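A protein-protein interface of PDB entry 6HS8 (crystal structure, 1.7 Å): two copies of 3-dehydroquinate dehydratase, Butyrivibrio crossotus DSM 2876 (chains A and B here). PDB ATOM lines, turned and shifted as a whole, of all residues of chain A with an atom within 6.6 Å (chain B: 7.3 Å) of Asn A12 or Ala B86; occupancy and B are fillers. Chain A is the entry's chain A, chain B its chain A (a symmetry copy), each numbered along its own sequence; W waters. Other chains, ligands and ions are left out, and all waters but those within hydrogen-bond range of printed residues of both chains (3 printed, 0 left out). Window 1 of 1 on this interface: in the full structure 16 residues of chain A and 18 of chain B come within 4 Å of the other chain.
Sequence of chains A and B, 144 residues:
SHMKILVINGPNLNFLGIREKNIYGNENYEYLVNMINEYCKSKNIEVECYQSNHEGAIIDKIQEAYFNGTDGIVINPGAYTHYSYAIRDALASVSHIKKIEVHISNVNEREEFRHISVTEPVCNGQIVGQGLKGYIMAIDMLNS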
ATOM      1  N   GLY A  10      -0.226   7.937 -10.173  1.00  0.00           N
ATOM      2  CA  GLY A  10      -1.376   7.787  -9.288  1.00  0.00           C
ATOM      3  C   GLY A  10      -1.418   6.511  -8.475  1.00  0.00           C
ATOM      4  O   GLY A  10      -0.388   5.845  -8.265  1.00  0.00           O
ATOM      5  N   PRO A  11      -2.631   6.089  -8.025  1.00  0.00           N
ATOM      6  CA  PRO A  11      -2.778   5.012  -7.064  1.00  0.00           C
ATOM      7  C   PRO A  11      -2.268   3.690  -7.631  1.00  0.00           C
ATOM      8  O   PRO A  11      -2.314   3.433  -8.851  1.00  0.00           O
ATOM      9  CB  PRO A  11      -4.270   4.989  -6.734  1.00  0.00           C
ATOM     10  CG  PRO A  11      -4.884   5.600  -7.970  1.00  0.00           C
ATOM     11  CD  PRO A  11      -3.927   6.701  -8.371  1.00  0.00           C
ATOM     12  N   ASN A  12      -1.659   2.900  -6.741  1.00  0.00           N
ATOM     13  CA  ASN A  12      -1.259   1.527  -7.014  1.00  0.00           C
ATOM     14  C   ASN A  12       0.031   1.403  -7.852  1.00  0.00           C
ATOM     15  O   ASN A  12       0.612   0.302  -7.889  1.00  0.00           O
ATOM     16  CB  ASN A  12      -2.414   0.726  -7.620  1.00  0.00           C
ATOM     17  CG  ASN A  12      -3.683   0.718  -6.796  1.00  0.00           C
ATOM     18  OD1 ASN A  12      -3.703   0.186  -5.669  1.00  0.00           O
ATOM     19  ND2 ASN A  12      -4.786   1.255  -7.362  1.00  0.00           N
ATOM     20  N   LEU A  13       0.495   2.467  -8.502  1.00  0.00           N
ATOM     21  CA  LEU A  13       1.633   2.374  -9.429  1.00  0.00           C
ATOM     22  C   LEU A  13       2.956   2.234  -8.635  1.00  0.00           C
ATOM     23  O   LEU A  13       3.898   1.696  -9.169  1.00  0.00           O
ATOM     24  CB  LEU A  13       1.610   3.582 -10.356  1.00  0.00           C
ATOM     25  CG  LEU A  13       0.536   3.435 -11.439  1.00  0.00           C
ATOM     26  CD1 LEU A  13       0.046   4.754 -11.884  1.00  0.00           C
ATOM     27  CD2 LEU A  13       1.085   2.613 -12.607  1.00  0.00           C
ATOM     28  N   ASN A  14       2.941   2.525  -7.324  1.00  0.00           N
ATOM     29  CA  ASN A  14       4.080   2.138  -6.425  1.00  0.00           C
ATOM     30  C   ASN A  14       4.265   0.612  -6.339  1.00  0.00           C
ATOM     31  O   ASN A  14       5.342   0.189  -5.867  1.00  0.00           O
ATOM     32  CB  ASN A  14       3.979   2.815  -5.049  1.00  0.00           C
ATOM     33  CG  ASN A  14       2.736   2.447  -4.275  1.00  0.00           C
ATOM     34  OD1 ASN A  14       1.673   2.350  -4.868  1.00  0.00           O
ATOM     35  ND2 ASN A  14       2.861   2.290  -2.958  1.00  0.00           N
ATOM     36  N   PHE A  15       3.266  -0.216  -6.749  1.00  0.00           N
ATOM     37  CA  PHE A  15       3.353  -1.689  -6.750  1.00  0.00           C
ATOM     38  C   PHE A  15       3.727  -2.282  -8.119  1.00  0.00           C
ATOM     39  O   PHE A  15       3.671  -3.506  -8.310  1.00  0.00           O
ATOM     40  CB  PHE A  15       2.060  -2.323  -6.179  1.00  0.00           C
ATOM     41  CG  PHE A  15       2.022  -2.541  -4.669  1.00  0.00           C
ATOM     42  CD1 PHE A  15       2.816  -1.809  -3.785  1.00  0.00           C
ATOM     43  CD2 PHE A  15       1.151  -3.468  -4.126  1.00  0.00           C
ATOM     44  CE1 PHE A  15       2.759  -2.034  -2.413  1.00  0.00           C
ATOM     45  CE2 PHE A  15       1.111  -3.706  -2.752  1.00  0.00           C
ATOM     46  CZ  PHE A  15       1.912  -2.992  -1.903  1.00  0.00           C
ATOM     47  N   LEU A  16       4.204  -1.449  -9.026  1.00  0.00           N
ATOM     48  CA  LEU A  16       4.746  -1.907 -10.291  1.00  0.00           C
ATOM     49  C   LEU A  16       5.768  -3.019 -10.067  1.00  0.00           C
ATOM     50  O   LEU A  16       6.667  -2.944  -9.188  1.00  0.00           O
ATOM     51  CB  LEU A  16       5.477  -0.772 -10.992  1.00  0.00           C
ATOM     52  CG  LEU A  16       4.670   0.033 -11.991  1.00  0.00           C
ATOM     53  CD1 LEU A  16       5.491   1.212 -12.494  1.00  0.00           C
ATOM     54  CD2 LEU A  16       4.238  -0.860 -13.153  1.00  0.00           C
ATOM     55  N   GLN A  51       4.552  10.104  -6.338  1.00  0.00           N
ATOM     56  CA  GLN A  51       3.446   9.117  -6.392  1.00  0.00           C
ATOM     57  C   GLN A  51       2.589   9.309  -5.144  1.00  0.00           C
ATOM     58  O   GLN A  51       3.140   9.530  -4.043  1.00  0.00           O
ATOM     59  CB  GLN A  51       4.001   7.701  -6.514  1.00  0.00           C
ATOM     60  CG  GLN A  51       2.966   6.588  -6.765  1.00  0.00           C
ATOM     61  CD  GLN A  51       2.278   6.099  -5.495  1.00  0.00           C
ATOM     62  OE1 GLN A  51       2.857   6.054  -4.375  1.00  0.00           O
ATOM     63  NE2 GLN A  51       1.036   5.624  -5.654  1.00  0.00           N
ATOM     64  N   SER A  52       1.284   9.083  -5.284  1.00  0.00           N
ATOM     65  CA  SER A  52       0.358   9.019  -4.169  1.00  0.00           C
ATOM     66  C   SER A  52      -0.850   8.146  -4.558  1.00  0.00           C
ATOM     67  O   SER A  52      -1.308   8.167  -5.705  1.00  0.00           O
ATOM     68  CB  SER A  52      -0.125  10.416  -3.738  1.00  0.00           C
ATOM     69  OG  SER A  52      -1.019  10.351  -2.617  1.00  0.00           O
ATOM     70  N   ASN A  53      -1.422   7.482  -3.560  1.00  0.00           N
ATOM     71  CA  ASN A  53      -2.747   6.831  -3.711  1.00  0.00           C
ATOM     72  C   ASN A  53      -3.924   7.795  -3.503  1.00  0.00           C
ATOM     73  O   ASN A  53      -5.094   7.389  -3.731  1.00  0.00           O
ATOM     74  CB  ASN A  53      -2.859   5.639  -2.773  1.00  0.00           C
ATOM     75  CG  ASN A  53      -1.794   4.596  -3.057  1.00  0.00           C
ATOM     76  OD1 ASN A  53      -1.434   4.349  -4.212  1.00  0.00           O
ATOM     77  ND2 ASN A  53      -1.281   3.981  -2.006  1.00  0.00           N
ATOM     78  N   ALA A  79      -5.906   4.282 -11.993  1.00  0.00           N
ATOM     79  CA  ALA A  79      -7.343   4.038 -12.084  1.00  0.00           C
ATOM     80  C   ALA A  79      -8.119   5.368 -12.105  1.00  0.00           C
ATOM     81  O   ALA A  79      -9.229   5.375 -12.632  1.00  0.00           O
ATOM     82  CB  ALA A  79      -7.811   3.111 -10.991  1.00  0.00           C
ATOM     83  N   TYR A  80      -7.576   6.464 -11.516  1.00  0.00           N
ATOM     84  CA  TYR A  80      -8.259   7.771 -11.522  1.00  0.00           C
ATOM     85  C   TYR A  80      -8.438   8.315 -12.956  1.00  0.00           C
ATOM     86  O   TYR A  80      -9.303   9.176 -13.177  1.00  0.00           O
ATOM     87  CB  TYR A  80      -7.560   8.808 -10.630  1.00  0.00           C
ATOM     88  CG  TYR A  80      -7.538   8.516  -9.144  1.00  0.00           C
ATOM     89  CD1 TYR A  80      -8.605   7.928  -8.494  1.00  0.00           C
ATOM     90  CD2 TYR A  80      -6.446   8.851  -8.355  1.00  0.00           C
ATOM     91  CE1 TYR A  80      -8.604   7.692  -7.125  1.00  0.00           C
ATOM     92  CE2 TYR A  80      -6.421   8.636  -6.978  1.00  0.00           C
ATOM     93  CZ  TYR A  80      -7.501   8.035  -6.350  1.00  0.00           C
ATOM     94  OH  TYR A  80      -7.509   7.719  -5.031  1.00  0.00           O
ATOM     95  N   TYR A  83     -12.262   8.083 -14.058  1.00  0.00           N
ATOM     96  CA  TYR A  83     -13.365   8.728 -13.358  1.00  0.00           C
ATOM     97  C   TYR A  83     -13.063  10.043 -12.637  1.00  0.00           C
ATOM     98  O   TYR A  83     -13.997  10.723 -12.286  1.00  0.00           O
ATOM     99  CB  TYR A  83     -14.016   7.751 -12.375  1.00  0.00           C
ATOM    100  CG  TYR A  83     -13.215   7.239 -11.188  1.00  0.00           C
ATOM    101  CD1 TYR A  83     -12.206   6.292 -11.350  1.00  0.00           C
ATOM    102  CD2 TYR A  83     -13.472   7.694  -9.901  1.00  0.00           C
ATOM    103  CE1 TYR A  83     -11.505   5.774 -10.260  1.00  0.00           C
ATOM    104  CE2 TYR A  83     -12.757   7.199  -8.800  1.00  0.00           C
ATOM    105  CZ  TYR A  83     -11.800   6.219  -8.973  1.00  0.00           C
ATOM    106  OH  TYR A  83     -11.101   5.636  -7.917  1.00  0.00           O
ATOM    107  N   GLU B  55     -10.522   7.567   0.429  1.00  0.00           N
ATOM    108  CA  GLU B  55     -10.212   6.540  -0.612  1.00  0.00           C
ATOM    109  C   GLU B  55      -8.709   6.171  -0.566  1.00  0.00           C
ATOM    110  O   GLU B  55      -8.347   4.997  -0.560  1.00  0.00           O
ATOM    111  CB  GLU B  55     -10.735   7.103  -1.939  1.00  0.00           C
ATOM    112  CG  GLU B  55     -10.576   6.185  -3.125  1.00  0.00           C
ATOM    113  CD  GLU B  55     -11.109   6.806  -4.428  1.00  0.00           C
ATOM    114  OE1 GLU B  55     -11.142   8.058  -4.511  1.00  0.00           O
ATOM    115  OE2 GLU B  55     -11.413   6.039  -5.359  1.00  0.00           O
ATOM    116  N   GLY B  56      -7.819   7.178  -0.536  1.00  0.00           N
ATOM    117  CA  GLY B  56      -6.398   6.942  -0.552  1.00  0.00           C
ATOM    118  C   GLY B  56      -5.898   6.214   0.688  1.00  0.00           C
ATOM    119  O   GLY B  56      -4.956   5.456   0.609  1.00  0.00           O
ATOM    120  N   ILE B  59      -6.650   2.526   0.271  1.00  0.00           N
ATOM    121  CA  ILE B  59      -5.663   1.906  -0.635  1.00  0.00           C
ATOM    122  C   ILE B  59      -4.337   1.637   0.134  1.00  0.00           C
ATOM    123  O   ILE B  59      -3.741   0.555   0.053  1.00  0.00           O
ATOM    124  CB  ILE B  59      -5.478   2.736  -1.902  1.00  0.00           C
ATOM    125  CG1 ILE B  59      -6.785   2.807  -2.706  1.00  0.00           C
ATOM    126  CG2 ILE B  59      -4.283   2.234  -2.721  1.00  0.00           C
ATOM    127  CD1 ILE B  59      -6.844   3.899  -3.753  1.00  0.00           C
ATOM    128  N   ASP B  60      -3.876   2.639   0.866  1.00  0.00           N
ATOM    129  CA  ASP B  60      -2.618   2.544   1.664  1.00  0.00           C
ATOM    130  C   ASP B  60      -2.709   1.339   2.624  1.00  0.00           C
ATOM    131  O   ASP B  60      -1.737   0.557   2.772  1.00  0.00           O
ATOM    132  CB  ASP B  60      -2.377   3.818   2.507  1.00  0.00           C
ATOM    133  CG  ASP B  60      -2.092   5.115   1.779  1.00  0.00           C
ATOM    134  OD1 ASP B  60      -1.644   5.063   0.580  1.00  0.00           O
ATOM    135  OD2 ASP B  60      -2.221   6.193   2.483  1.00  0.00           O
ATOM    136  N   ILE B  62      -4.688  -1.371   2.380  1.00  0.00           N
ATOM    137  CA  ILE B  62      -4.637  -2.604   1.547  1.00  0.00           C
ATOM    138  C   ILE B  62      -3.199  -2.936   1.171  1.00  0.00           C
ATOM    139  O   ILE B  62      -2.802  -4.111   1.343  1.00  0.00           O
ATOM    140  CB  ILE B  62      -5.569  -2.511   0.326  1.00  0.00           C
ATOM    141  CG1 ILE B  62      -7.042  -2.464   0.771  1.00  0.00           C
ATOM    142  CG2 ILE B  62      -5.276  -3.676  -0.614  1.00  0.00           C
ATOM    143  CD1 ILE B  62      -7.986  -1.980  -0.340  1.00  0.00           C
ATOM    144  N   GLN B  63      -2.393  -1.946   0.746  1.00  0.00           N
ATOM    145  CA  GLN B  63      -0.992  -2.157   0.411  1.00  0.00           C
ATOM    146  C   GLN B  63      -0.199  -2.662   1.636  1.00  0.00           C
ATOM    147  O   GLN B  63       0.656  -3.618   1.484  1.00  0.00           O
ATOM    148  CB  GLN B  63      -0.355  -0.905  -0.180  1.00  0.00           C
ATOM    149  CG  GLN B  63      -0.977  -0.497  -1.535  1.00  0.00           C
ATOM    150  CD  GLN B  63      -0.175   0.565  -2.247  1.00  0.00           C
ATOM    151  OE1 GLN B  63       0.371   1.466  -1.607  1.00  0.00           O
ATOM    152  NE2 GLN B  63      -0.131   0.490  -3.570  1.00  0.00           N
ATOM    153  N   TYR B  83     -18.114   3.193  -7.559  1.00  0.00           N
ATOM    154  CA  TYR B  83     -17.297   3.958  -8.492  1.00  0.00           C
ATOM    155  C   TYR B  83     -15.779   3.888  -8.313  1.00  0.00           C
ATOM    156  O   TYR B  83     -15.084   4.283  -9.218  1.00  0.00           O
ATOM    157  CB  TYR B  83     -17.735   5.424  -8.507  1.00  0.00           C
ATOM    158  CG  TYR B  83     -17.564   6.269  -7.254  1.00  0.00           C
ATOM    159  CD1 TYR B  83     -18.399   6.105  -6.150  1.00  0.00           C
ATOM    160  CD2 TYR B  83     -16.574   7.240  -7.175  1.00  0.00           C
ATOM    161  CE1 TYR B  83     -18.287   6.915  -5.019  1.00  0.00           C
ATOM    162  CE2 TYR B  83     -16.436   8.043  -6.033  1.00  0.00           C
ATOM    163  CZ  TYR B  83     -17.308   7.905  -4.972  1.00  0.00           C
ATOM    164  OH  TYR B  83     -17.269   8.715  -3.838  1.00  0.00           O
ATOM    165  N   SER B  84     -15.244   3.418  -7.167  1.00  0.00           N
ATOM    166  CA  SER B  84     -13.773   3.478  -6.936  1.00  0.00           C
ATOM    167  C   SER B  84     -13.004   2.373  -7.669  1.00  0.00           C
ATOM    168  O   SER B  84     -12.631   1.325  -7.058  1.00  0.00           O
ATOM    169  CB  SER B  84     -13.465   3.432  -5.445  1.00  0.00           C
ATOM    170  OG  SER B  84     -12.043   3.523  -5.231  1.00  0.00           O
ATOM    171  N   TYR B  85     -12.672   2.608  -8.951  1.00  0.00           N
ATOM    172  CA  TYR B  85     -11.782   1.669  -9.647  1.00  0.00           C
ATOM    173  C   TYR B  85     -10.379   1.663  -8.968  1.00  0.00           C
ATOM    174  O   TYR B  85      -9.623   0.674  -9.119  1.00  0.00           O
ATOM    175  CB  TYR B  85     -11.695   1.995 -11.129  1.00  0.00           C
ATOM    176  CG  TYR B  85     -13.001   1.747 -11.856  1.00  0.00           C
ATOM    177  CD1 TYR B  85     -13.434   0.447 -12.070  1.00  0.00           C
ATOM    178  CD2 TYR B  85     -13.748   2.798 -12.358  1.00  0.00           C
ATOM    179  CE1 TYR B  85     -14.617   0.198 -12.766  1.00  0.00           C
ATOM    180  CE2 TYR B  85     -14.925   2.559 -13.074  1.00  0.00           C
ATOM    181  CZ  TYR B  85     -15.338   1.257 -13.272  1.00  0.00           C
ATOM    182  OH  TYR B  85     -16.503   1.055 -13.990  1.00  0.00           O
ATOM    183  N   ALA B  86      -9.995   2.727  -8.228  1.00  0.00           N
ATOM    184  CA  ALA B  86      -8.671   2.739  -7.540  1.00  0.00           C
ATOM    185  C   ALA B  86      -8.636   1.687  -6.402  1.00  0.00           C
ATOM    186  O   ALA B  86      -7.635   0.957  -6.229  1.00  0.00           O
ATOM    187  CB  ALA B  86      -8.331   4.136  -7.033  1.00  0.00           C
ATOM    188  N   ILE B  87      -9.731   1.550  -5.640  1.00  0.00           N
ATOM    189  CA  ILE B  87      -9.833   0.529  -4.584  1.00  0.00           C
ATOM    190  C   ILE B  87      -9.925  -0.866  -5.229  1.00  0.00           C
ATOM    191  O   ILE B  87      -9.286  -1.806  -4.735  1.00  0.00           O
ATOM    192  CB  ILE B  87     -10.983   0.807  -3.579  1.00  0.00           C
ATOM    193  CG1 ILE B  87     -10.675   2.030  -2.714  1.00  0.00           C
ATOM    194  CG2 ILE B  87     -11.258  -0.454  -2.739  1.00  0.00           C
ATOM    195  CD1 ILE B  87     -11.832   2.602  -1.894  1.00  0.00           C
ATOM    196  N   ARG B  88     -10.649  -1.017  -6.360  1.00  0.00           N
ATOM    197  CA  ARG B  88     -10.676  -2.294  -7.087  1.00  0.00           C
ATOM    198  C   ARG B  88      -9.235  -2.719  -7.452  1.00  0.00           C
ATOM    199  O   ARG B  88      -8.788  -3.855  -7.154  1.00  0.00           O
ATOM    200  CB  ARG B  88     -11.484  -2.157  -8.382  1.00  0.00           C
ATOM    201  CG  ARG B  88     -11.419  -3.377  -9.302  1.00  0.00           C
ATOM    202  CD  ARG B  88     -11.699  -2.957 -10.735  1.00  0.00           C
ATOM    203  NE  ARG B  88     -11.747  -4.086 -11.667  1.00  0.00           N
ATOM    204  CZ  ARG B  88     -12.868  -4.539 -12.277  1.00  0.00           C
ATOM    205  NH1 ARG B  88     -14.083  -4.105 -11.938  1.00  0.00           N
ATOM    206  NH2 ARG B  88     -12.741  -5.409 -13.284  1.00  0.00           N
ATOM    207  N   ASP B  89      -8.464  -1.800  -8.024  1.00  0.00           N
ATOM    208  CA  ASP B  89      -7.102  -2.103  -8.454  1.00  0.00           C
ATOM    209  C   ASP B  89      -6.183  -2.411  -7.257  1.00  0.00           C
ATOM    210  O   ASP B  89      -5.246  -3.215  -7.388  1.00  0.00           O
ATOM    211  CB  ASP B  89      -6.542  -1.047  -9.404  1.00  0.00           C
ATOM    212  CG  ASP B  89      -6.981  -1.229 -10.861  1.00  0.00           C
ATOM    213  OD1 ASP B  89      -7.788  -2.183 -11.134  1.00  0.00           O
ATOM    214  OD2 ASP B  89      -6.602  -0.376 -11.689  1.00  0.00           O
ATOM    215  N   ALA B  90      -6.417  -1.768  -6.104  1.00  0.00           N
ATOM    216  CA  ALA B  90      -5.654  -2.094  -4.886  1.00  0.00           C
ATOM    217  C   ALA B  90      -5.936  -3.533  -4.455  1.00  0.00           C
ATOM    218  O   ALA B  90      -5.001  -4.336  -4.171  1.00  0.00           O
ATOM    219  CB  ALA B  90      -5.967  -1.090  -3.797  1.00  0.00           C
ATOM    220  N   LEU B  91      -7.219  -3.920  -4.470  1.00  0.00           N
ATOM    221  CA  LEU B  91      -7.575  -5.334  -4.116  1.00  0.00           C
ATOM    222  C   LEU B  91      -6.942  -6.362  -5.090  1.00  0.00           C
ATOM    223  O   LEU B  91      -6.461  -7.444  -4.645  1.00  0.00           O
ATOM    224  CB  LEU B  91      -9.103  -5.454  -4.029  1.00  0.00           C
ATOM    225  CG  LEU B  91      -9.812  -4.683  -2.897  1.00  0.00           C
ATOM    226  CD1 LEU B  91     -11.329  -4.712  -3.032  1.00  0.00           C
ATOM    227  CD2 LEU B  91      -9.402  -5.203  -1.519  1.00  0.00           C
ATOM    228  N   ALA B  92      -6.914  -6.037  -6.397  1.00  0.00           N
ATOM    229  CA  ALA B  92      -6.364  -6.914  -7.416  1.00  0.00           C
ATOM    230  C   ALA B  92      -4.849  -7.067  -7.222  1.00  0.00           C
ATOM    231  O   ALA B  92      -4.258  -8.118  -7.577  1.00  0.00           O
ATOM    232  CB  ALA B  92      -6.679  -6.369  -8.796  1.00  0.00           C
ATOM    233  N   SER B  93      -4.204  -6.022  -6.696  1.00  0.00           N
ATOM    234  CA  SER B  93      -2.745  -5.991  -6.535  1.00  0.00           C
ATOM    235  C   SER B  93      -2.288  -6.940  -5.405  1.00  0.00           C
ATOM    236  O   SER B  93      -1.062  -7.230  -5.290  1.00  0.00           O
ATOM    237  CB  SER B  93      -2.219  -4.584  -6.322  1.00  0.00           C
ATOM    238  OG  SER B  93      -2.466  -4.158  -4.997  1.00  0.00           O
ATOM    239  N   VAL B 118     -17.965  -2.096  -8.523  1.00  0.00           N
ATOM    240  CA  VAL B 118     -16.735  -2.131  -9.307  1.00  0.00           C
ATOM    241  C   VAL B 118     -15.662  -2.970  -8.596  1.00  0.00           C
ATOM    242  O   VAL B 118     -14.694  -3.340  -9.229  1.00  0.00           O
ATOM    243  CB  VAL B 118     -16.208  -0.728  -9.622  1.00  0.00           C
ATOM    244  CG1 VAL B 118     -17.261   0.094 -10.296  1.00  0.00           C
ATOM    245  CG2 VAL B 118     -15.623  -0.021  -8.399  1.00  0.00           C
ATOM    246  N   THR B 119     -15.862  -3.265  -7.303  1.00  0.00           N
ATOM    247  CA  THR B 119     -14.934  -4.040  -6.534  1.00  0.00           C
ATOM    248  C   THR B 119     -15.227  -5.559  -6.587  1.00  0.00           C
ATOM    249  O   THR B 119     -14.312  -6.380  -6.501  1.00  0.00           O
ATOM    250  CB  THR B 119     -14.859  -3.518  -5.095  1.00  0.00           C
ATOM    251  OG1 THR B 119     -16.189  -3.424  -4.585  1.00  0.00           O
ATOM    252  CG2 THR B 119     -14.152  -2.183  -4.984  1.00  0.00           C
HETATM  253  O   HOH W   1      -1.563  -1.477  -5.020  1.00  0.00           O
HETATM  254  O   HOH W   2      -8.224   9.573  -2.709  1.00  0.00           O
HETATM  255  O   HOH W   3      -0.317   7.069  -0.775  1.00  0.00           O
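The backbone NH of Asn A12 lies within hydrogen-bond range of the side-chain amide oxygen of Asn A53 (2.9 Å).
The side-chain hydroxyl (OH) of Tyr A80 lies within hydrogen-bond range of the backbone carbonyl oxygen (O) of Asn A53, 2.8 Å away.
The side-chain amide nitrogen (NE2) of Gln A51 sits at hydrogen-bond distance from the side-chain amide oxygen (OD1) of Asn A14, at 3.4 Å.
NE2 of Gln A51 lies within hydrogen-bond range of OD1 of Asn A53 (3.1 Å).
OE2 of Glu B55 is in hydrogen-bond range of OG of Ser B84.
O of Ala B90 is in hydrogen-bond range of OG of Ser B93.
Tyr A83 touches its own counterpart, Tyr B83.
Of the 23 pairs that touch across the chains among the printed residues, 1 has its exchanged pair printed and touching as well.
Water W3 bridges OD1 of Asp B60 (2.8 Å) and N of Asn A53 (3.0 Å).
Water W1 lies within hydrogen-bond range of OD1 of Asn A12 (2.8 Å), OG of Ser B93 (2.8 Å) and NE2 of Gln B63 (2.8 Å).
Water W2 lies within hydrogen-bond range of OH of Tyr A80 (3.1 Å) and N of Gly B56 (3.3 Å).
Ile B59 touches Asn A12.
Asp B89 touches Asn A12 (CB to ND2, 3.5 Å).
Phe A15 touches Gln B63.
CD2 of Phe A15 touches OG of Ser B93, at 3.8 Å.
Gly B56 touches Asn A53 (CA to O, 3.5 Å).
CG of Asn A53 touches CG2 of Ile B59, at 3.4 Å.
Ala A79 touches Ala B86 (CB to N, 3.5 Å).
CE1 of Tyr A80 touches OE1 of Glu B55, 3.7 Å away.
Tyr A80 touches Ala B86 (CE1 to CB, 3.6 Å).
Tyr A83 touches Tyr B85.
Hydrophobic or aromatic side chains of chain A that line the printed part of chain B: Pro A11, Phe A15, Ala A79, Tyr A80 and Tyr A83.
Of the 19 printed residues of chain B, 12 touch a printed residue of chain A.
Printed residues of chain B that touch a printed residue of chain A: Glu B55, Gly B56, Ile B59, Asp B60, Gln B63, Tyr B83, Ser B84, Tyr B85, Ala B86, Asp B89, Ala B90 and Ser B93.
Along chain B the printed residues that touch a printed residue of chain A span positions 55 to 93.
Among the printed residues, no Asp or Glu carboxylate lies within 4 Å of a Lys or Arg side-chain nitrogen of the other chain.
The side-chain amide oxygen (OD1) of Asn A12 lies close to the backbone NH (N) of Ala B90 (3.4 Å).
OD1 of Asp B60 lies within hydrogen-bond range of ND2 of Asn A53, 2.8 Å away.
The side-chain amide oxygen of Gln B63 sits at hydrogen-bond distance from the side-chain amide nitrogen of Asn A53.
N of Ala B86 lies within hydrogen-bond range of OH of Tyr A83.
The side-chain carboxylate of Glu B55 sits at hydrogen-bond distance from the side-chain hydroxyl of Tyr A83, at 2.6 Å.
The side-chain amide nitrogen of Asn A12 lies within hydrogen-bond range of the backbone carbonyl oxygen of Ala B86 (3.1 Å).
The side-chain amide nitrogen (NE2) of Gln B63 lies within hydrogen-bond range of the side-chain amide oxygen (OD1) of Asn A14, at 2.9 Å.
Of chain B, only Ile B59, Gln B63, Ala B86, Asp B89 and Ala B90 come within 4 Å of Asn A12.
Of the printed residues of chain B, Phe A15 touches Gln B63 (3.5 Å) and Ser B93 (3.8 Å).
Printed residues of chain A within 4 Å of Ile B59: Asn A12 (3.6 Å) and Asn A53 (3.4 Å).
Ala B86 touches five residues of chain A.
The nearest residue of chain B that does not touch Asn A12 is Ser B93 (4.6 Å).
The nearest residue of chain A that does not touch Ala B86 is Asn A53 (5.7 Å).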
